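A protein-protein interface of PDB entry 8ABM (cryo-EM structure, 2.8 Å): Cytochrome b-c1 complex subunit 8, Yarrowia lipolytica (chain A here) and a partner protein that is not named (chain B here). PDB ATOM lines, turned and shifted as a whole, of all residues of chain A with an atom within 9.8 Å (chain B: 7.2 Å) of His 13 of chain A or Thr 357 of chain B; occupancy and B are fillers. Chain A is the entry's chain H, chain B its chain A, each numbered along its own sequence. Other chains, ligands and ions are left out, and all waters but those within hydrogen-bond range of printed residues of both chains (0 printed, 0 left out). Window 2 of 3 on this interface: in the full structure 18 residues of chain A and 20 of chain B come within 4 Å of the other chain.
The side-chain carboxylate (OE2) of Glu 457 of chain B sits at hydrogen-bond distance from the backbone NH (N) of Gly 12 of chain A (2.9 Å). OE2 of Glu 457 of chain B is in hydrogen-bond range of N of His 13 of chain A (2.9 Å). The side-chain carboxylate (OE2) of Glu 457 of chain B sits at hydrogen-bond distance from the backbone NH (N) of Met 14 of chain A, 2.6 Å away.
The side-chain hydroxyl (OG1) of Thr 357 of chain B lies within hydrogen-bond range of the side-chain amide oxygen (OD1) of Asn 355 of chain B. The backbone carbonyl oxygen (O) of Met 14 of chain A sits at hydrogen-bond distance from the backbone NH (N) of Gly 9 of chain A (2.9 Å).
Glu 457 of chain B touches Trp 10 of chain A (OE2 to O, 3.6 Å). Glu 457 of chain B touches Trp 11 of chain A (O to CE3, 3.8 Å). Gly 12 of chain A touches Thr 356 of chain B. CA of Gly 458 of chain B touches N of Gly 12 of chain A (3.9 Å). Thr 357 of chain B touches His 13 of chain A.
Of the printed residues of chain B, Trp 10 of chain A touches Glu 457 (3.6 Å). Printed residues of chain B within 4 Å of Trp 11 of chain A: Glu 457. Thr 356 of chain B touches one residue of chain A. Of chain A, only His 13 (3.97 Å) comes within 4 Å of Thr 357 of chain B. Asp 360 of chain B touches none of the printed residues of chain A. Of the printed residues of chain A, Gly 458 of chain B touches Gly 12.
Hydrophobic or aromatic side chains of chain A within 4 Å of the printed part of chain B: Trp 11, His 13 and Met 14. Among the printed residues, 8 pairs touch across the chains. Among the printed residues, no Asp or Glu carboxylate lies within 4 Å of a Lys or Arg side-chain nitrogen of the other chain.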
ATOM      1  N   TYR A   7      11.981  24.713  -1.185  1.00  0.00           N
ATOM      2  CA  TYR A   7      10.783  24.258  -0.271  1.00  0.00           C
ATOM      3  C   TYR A   7      10.255  22.858  -0.591  1.00  0.00           C
ATOM      4  O   TYR A   7       9.593  22.206   0.227  1.00  0.00           O
ATOM      5  CB  TYR A   7       9.585  25.215  -0.297  1.00  0.00           C
ATOM      6  CG  TYR A   7       9.792  26.463   0.518  1.00  0.00           C
ATOM      7  CD1 TYR A   7      10.069  26.402   1.878  1.00  0.00           C
ATOM      8  CD2 TYR A   7       9.793  27.711  -0.090  1.00  0.00           C
ATOM      9  CE1 TYR A   7      10.322  27.551   2.616  1.00  0.00           C
ATOM     10  CE2 TYR A   7      10.044  28.868   0.633  1.00  0.00           C
ATOM     11  CZ  TYR A   7      10.302  28.790   1.993  1.00  0.00           C
ATOM     12  OH  TYR A   7      10.535  29.935   2.705  1.00  0.00           O
ATOM     13  N   MET A   8      10.477  22.408  -1.820  1.00  0.00           N
ATOM     14  CA  MET A   8      10.299  21.001  -2.117  1.00  0.00           C
ATOM     15  C   MET A   8      11.596  20.502  -2.730  1.00  0.00           C
ATOM     16  O   MET A   8      12.184  21.175  -3.578  1.00  0.00           O
ATOM     17  CB  MET A   8       9.147  20.801  -3.098  1.00  0.00           C
ATOM     18  CG  MET A   8       8.919  19.344  -3.419  1.00  0.00           C
ATOM     19  SD  MET A   8       7.749  19.094  -4.757  1.00  0.00           S
ATOM     20  CE  MET A   8       8.637  19.775  -6.161  1.00  0.00           C
ATOM     21  N   GLY A   9      12.029  19.306  -2.326  1.00  0.00           N
ATOM     22  CA  GLY A   9      13.222  18.756  -2.936  1.00  0.00           C
ATOM     23  C   GLY A   9      12.871  17.809  -4.069  1.00  0.00           C
ATOM     24  O   GLY A   9      12.130  18.137  -4.992  1.00  0.00           O
ATOM     25  N   TRP A  10      13.447  16.627  -3.984  1.00  0.00           N
ATOM     26  CA  TRP A  10      13.201  15.580  -4.946  1.00  0.00           C
ATOM     27  C   TRP A  10      13.326  14.268  -4.195  1.00  0.00           C
ATOM     28  O   TRP A  10      13.658  14.268  -3.010  1.00  0.00           O
ATOM     29  CB  TRP A  10      14.213  15.672  -6.083  1.00  0.00           C
ATOM     30  CG  TRP A  10      13.684  15.048  -7.336  1.00  0.00           C
ATOM     31  CD1 TRP A  10      14.048  13.856  -7.899  1.00  0.00           C
ATOM     32  CD2 TRP A  10      12.623  15.571  -8.157  1.00  0.00           C
ATOM     33  NE1 TRP A  10      13.313  13.614  -9.034  1.00  0.00           N
ATOM     34  CE2 TRP A  10      12.424  14.648  -9.215  1.00  0.00           C
ATOM     35  CE3 TRP A  10      11.825  16.727  -8.098  1.00  0.00           C
ATOM     36  CZ2 TRP A  10      11.465  14.863 -10.211  1.00  0.00           C
ATOM     37  CZ3 TRP A  10      10.885  16.939  -9.088  1.00  0.00           C
ATOM     38  CH2 TRP A  10      10.708  16.017 -10.129  1.00  0.00           C
ATOM     39  N   TRP A  11      13.038  13.168  -4.881  1.00  0.00           N
ATOM     40  CA  TRP A  11      13.025  11.895  -4.197  1.00  0.00           C
ATOM     41  C   TRP A  11      14.362  11.662  -3.513  1.00  0.00           C
ATOM     42  O   TRP A  11      15.410  11.781  -4.141  1.00  0.00           O
ATOM     43  CB  TRP A  11      12.757  10.814  -5.220  1.00  0.00           C
ATOM     44  CG  TRP A  11      11.458  11.037  -5.914  1.00  0.00           C
ATOM     45  CD1 TRP A  11      11.269  11.541  -7.167  1.00  0.00           C
ATOM     46  CD2 TRP A  11      10.154  10.766  -5.379  1.00  0.00           C
ATOM     47  NE1 TRP A  11       9.934  11.572  -7.461  1.00  0.00           N
ATOM     48  CE2 TRP A  11       9.223  11.113  -6.384  1.00  0.00           C
ATOM     49  CE3 TRP A  11       9.685  10.269  -4.153  1.00  0.00           C
ATOM     50  CZ2 TRP A  11       7.845  10.979  -6.195  1.00  0.00           C
ATOM     51  CZ3 TRP A  11       8.323  10.135  -3.968  1.00  0.00           C
ATOM     52  CH2 TRP A  11       7.420  10.488  -4.976  1.00  0.00           C
ATOM     53  N   GLY A  12      14.303  11.333  -2.225  1.00  0.00           N
ATOM     54  CA  GLY A  12      15.532  11.116  -1.490  1.00  0.00           C
ATOM     55  C   GLY A  12      15.927  12.324  -0.647  1.00  0.00           C
ATOM     56  O   GLY A  12      16.607  12.158   0.365  1.00  0.00           O
ATOM     57  N   HIS A  13      15.503  13.526  -1.048  1.00  0.00           N
ATOM     58  CA  HIS A  13      15.765  14.701  -0.235  1.00  0.00           C
ATOM     59  C   HIS A  13      14.581  15.656  -0.367  1.00  0.00           C
ATOM     60  O   HIS A  13      14.743  16.819  -0.733  1.00  0.00           O
ATOM     61  CB  HIS A  13      17.146  15.292  -0.589  1.00  0.00           C
ATOM     62  CG  HIS A  13      17.253  15.682  -2.024  1.00  0.00           C
ATOM     63  ND1 HIS A  13      17.445  14.750  -3.022  1.00  0.00           N
ATOM     64  CD2 HIS A  13      17.136  16.882  -2.640  1.00  0.00           C
ATOM     65  CE1 HIS A  13      17.442  15.350  -4.193  1.00  0.00           C
ATOM     66  NE2 HIS A  13      17.258  16.665  -3.987  1.00  0.00           N
ATOM     67  N   MET A  14      13.384  15.150  -0.062  1.00  0.00           N
ATOM     68  CA  MET A  14      12.158  15.872  -0.352  1.00  0.00           C
ATOM     69  C   MET A  14      12.013  17.072   0.581  1.00  0.00           C
ATOM     70  O   MET A  14      11.402  18.066   0.202  1.00  0.00           O
ATOM     71  CB  MET A  14      10.934  14.969  -0.196  1.00  0.00           C
ATOM     72  CG  MET A  14       9.692  15.500  -0.889  1.00  0.00           C
ATOM     73  SD  MET A  14       9.876  15.406  -2.685  1.00  0.00           S
ATOM     74  CE  MET A  14      10.022  13.629  -2.872  1.00  0.00           C
ATOM     75  N   GLY A  15      12.590  16.995   1.783  1.00  0.00           N
ATOM     76  CA  GLY A  15      12.544  18.127   2.693  1.00  0.00           C
ATOM     77  C   GLY A  15      11.553  17.905   3.833  1.00  0.00           C
ATOM     78  O   GLY A  15      11.193  18.846   4.542  1.00  0.00           O
ATOM     79  N   SER A  16      11.141  16.645   4.010  1.00  0.00           N
ATOM     80  CA  SER A  16      10.413  16.197   5.185  1.00  0.00           C
ATOM     81  C   SER A  16      11.283  16.373   6.427  1.00  0.00           C
ATOM     82  O   SER A  16      12.498  16.187   6.366  1.00  0.00           O
ATOM     83  CB  SER A  16       9.995  14.761   5.012  1.00  0.00           C
ATOM     84  OG  SER A  16       9.389  14.248   6.193  1.00  0.00           O
ATOM     85  N   PRO A  17      10.700  16.721   7.597  1.00  0.00           N
ATOM     86  CA  PRO A  17      11.402  16.547   8.868  1.00  0.00           C
ATOM     87  C   PRO A  17      11.713  15.058   8.956  1.00  0.00           C
ATOM     88  O   PRO A  17      11.024  14.262   8.324  1.00  0.00           O
ATOM     89  CB  PRO A  17      10.333  16.883   9.908  1.00  0.00           C
ATOM     90  CG  PRO A  17       9.387  17.794   9.180  1.00  0.00           C
ATOM     91  CD  PRO A  17       9.352  17.285   7.758  1.00  0.00           C
ATOM     92  N   SER B 353      22.106  -0.195   0.691  1.00  0.00           N
ATOM     93  CA  SER B 353      22.576   0.928  -0.086  1.00  0.00           C
ATOM     94  C   SER B 353      22.627   2.154   0.805  1.00  0.00           C
ATOM     95  O   SER B 353      21.682   2.398   1.549  1.00  0.00           O
ATOM     96  CB  SER B 353      21.664   1.163  -1.259  1.00  0.00           C
ATOM     97  OG  SER B 353      22.074   2.319  -1.972  1.00  0.00           O
ATOM     98  N   GLU B 354      23.696   2.938   0.645  1.00  0.00           N
ATOM     99  CA  GLU B 354      23.775   4.269   1.220  1.00  0.00           C
ATOM    100  C   GLU B 354      23.425   5.337   0.187  1.00  0.00           C
ATOM    101  O   GLU B 354      23.397   6.521   0.506  1.00  0.00           O
ATOM    102  CB  GLU B 354      25.200   4.563   1.670  1.00  0.00           C
ATOM    103  CG  GLU B 354      25.667   3.724   2.840  1.00  0.00           C
ATOM    104  CD  GLU B 354      27.174   3.492   2.902  1.00  0.00           C
ATOM    105  OE1 GLU B 354      27.649   2.926   3.920  1.00  0.00           O
ATOM    106  OE2 GLU B 354      27.881   3.851   1.925  1.00  0.00           O
ATOM    107  N   ASN B 355      23.224   4.936  -1.065  1.00  0.00           N
ATOM    108  CA  ASN B 355      22.996   5.912  -2.113  1.00  0.00           C
ATOM    109  C   ASN B 355      21.513   6.239  -2.113  1.00  0.00           C
ATOM    110  O   ASN B 355      20.758   5.695  -2.910  1.00  0.00           O
ATOM    111  CB  ASN B 355      23.451   5.366  -3.465  1.00  0.00           C
ATOM    112  CG  ASN B 355      23.476   6.365  -4.608  1.00  0.00           C
ATOM    113  OD1 ASN B 355      22.900   7.451  -4.534  1.00  0.00           O
ATOM    114  ND2 ASN B 355      24.142   5.991  -5.688  1.00  0.00           N
ATOM    115  N   THR B 356      21.108   7.159  -1.251  1.00  0.00           N
ATOM    116  CA  THR B 356      19.688   7.262  -0.974  1.00  0.00           C
ATOM    117  C   THR B 356      18.934   8.020  -2.058  1.00  0.00           C
ATOM    118  O   THR B 356      17.711   7.924  -2.122  1.00  0.00           O
ATOM    119  CB  THR B 356      19.443   7.828   0.419  1.00  0.00           C
ATOM    120  OG1 THR B 356      20.153   9.067   0.450  1.00  0.00           O
ATOM    121  CG2 THR B 356      19.934   6.877   1.484  1.00  0.00           C
ATOM    122  N   THR B 357      19.663   8.719  -2.924  1.00  0.00           N
ATOM    123  CA  THR B 357      19.033   9.428  -4.023  1.00  0.00           C
ATOM    124  C   THR B 357      18.945   8.559  -5.276  1.00  0.00           C
ATOM    125  O   THR B 357      18.400   8.991  -6.290  1.00  0.00           O
ATOM    126  CB  THR B 357      19.750  10.755  -4.269  1.00  0.00           C
ATOM    127  OG1 THR B 357      21.053  10.392  -4.726  1.00  0.00           O
ATOM    128  CG2 THR B 357      19.829  11.578  -3.003  1.00  0.00           C
ATOM    129  N   GLN B 358      19.485   7.342  -5.240  1.00  0.00           N
ATOM    130  CA  GLN B 358      19.396   6.550  -6.451  1.00  0.00           C
ATOM    131  C   GLN B 358      18.855   5.169  -6.132  1.00  0.00           C
ATOM    132  O   GLN B 358      19.081   4.214  -6.875  1.00  0.00           O
ATOM    133  CB  GLN B 358      20.745   6.466  -7.138  1.00  0.00           C
ATOM    134  CG  GLN B 358      21.169   7.731  -7.851  1.00  0.00           C
ATOM    135  CD  GLN B 358      22.376   7.364  -8.673  1.00  0.00           C
ATOM    136  OE1 GLN B 358      23.515   7.528  -8.234  1.00  0.00           O
ATOM    137  NE2 GLN B 358      22.130   6.788  -9.845  1.00  0.00           N
ATOM    138  N   ILE B 359      18.099   5.091  -5.044  1.00  0.00           N
ATOM    139  CA  ILE B 359      17.420   3.858  -4.711  1.00  0.00           C
ATOM    140  C   ILE B 359      16.497   3.452  -5.859  1.00  0.00           C
ATOM    141  O   ILE B 359      16.377   2.266  -6.170  1.00  0.00           O
ATOM    142  CB  ILE B 359      16.678   4.038  -3.385  1.00  0.00           C
ATOM    143  CG1 ILE B 359      17.639   3.821  -2.225  1.00  0.00           C
ATOM    144  CG2 ILE B 359      15.484   3.106  -3.282  1.00  0.00           C
ATOM    145  CD1 ILE B 359      17.021   4.216  -0.942  1.00  0.00           C
ATOM    146  N   ASP B 360      15.852   4.449  -6.476  1.00  0.00           N
ATOM    147  CA  ASP B 360      14.967   4.204  -7.600  1.00  0.00           C
ATOM    148  C   ASP B 360      15.720   3.476  -8.706  1.00  0.00           C
ATOM    149  O   ASP B 360      15.196   2.498  -9.227  1.00  0.00           O
ATOM    150  CB  ASP B 360      14.272   5.475  -8.082  1.00  0.00           C
ATOM    151  CG  ASP B 360      15.205   6.544  -8.626  1.00  0.00           C
ATOM    152  OD1 ASP B 360      16.355   6.632  -8.144  1.00  0.00           O
ATOM    153  OD2 ASP B 360      14.766   7.288  -9.527  1.00  0.00           O
ATOM    154  N   ASP B 361      16.957   3.905  -9.012  1.00  0.00           N
ATOM    155  CA  ASP B 361      17.746   3.272 -10.055  1.00  0.00           C
ATOM    156  C   ASP B 361      18.127   1.860  -9.639  1.00  0.00           C
ATOM    157  O   ASP B 361      18.018   0.938 -10.438  1.00  0.00           O
ATOM    158  CB  ASP B 361      18.996   4.076 -10.404  1.00  0.00           C
ATOM    159  CG  ASP B 361      18.675   5.430 -11.007  1.00  0.00           C
ATOM    160  OD1 ASP B 361      17.845   5.483 -11.943  1.00  0.00           O
ATOM    161  OD2 ASP B 361      19.244   6.426 -10.526  1.00  0.00           O
ATOM    162  N   PRO B 455      16.412   4.925   5.279  1.00  0.00           N
ATOM    163  CA  PRO B 455      16.097   6.129   4.508  1.00  0.00           C
ATOM    164  C   PRO B 455      15.581   5.809   3.104  1.00  0.00           C
ATOM    165  O   PRO B 455      16.319   5.852   2.130  1.00  0.00           O
ATOM    166  CB  PRO B 455      17.471   6.790   4.559  1.00  0.00           C
ATOM    167  CG  PRO B 455      18.409   5.617   4.407  1.00  0.00           C
ATOM    168  CD  PRO B 455      17.843   4.607   5.367  1.00  0.00           C
ATOM    169  N   GLU B 457      12.876   7.145   1.472  1.00  0.00           N
ATOM    170  CA  GLU B 457      12.057   8.172   0.840  1.00  0.00           C
ATOM    171  C   GLU B 457      12.061   7.999  -0.680  1.00  0.00           C
ATOM    172  O   GLU B 457      11.036   8.183  -1.331  1.00  0.00           O
ATOM    173  CB  GLU B 457      12.580   9.565   1.185  1.00  0.00           C
ATOM    174  CG  GLU B 457      11.729  10.686   0.617  1.00  0.00           C
ATOM    175  CD  GLU B 457      12.260  12.077   0.918  1.00  0.00           C
ATOM    176  OE1 GLU B 457      11.899  12.647   1.975  1.00  0.00           O
ATOM    177  OE2 GLU B 457      13.037  12.587   0.092  1.00  0.00           O
ATOM    178  N   GLY B 458      13.222   7.641  -1.232  1.00  0.00           N
ATOM    179  CA  GLY B 458      13.398   7.540  -2.667  1.00  0.00           C
ATOM    180  C   GLY B 458      12.846   6.251  -3.265  1.00  0.00           C
ATOM    181  O   GLY B 458      12.903   6.071  -4.478  1.00  0.00           O
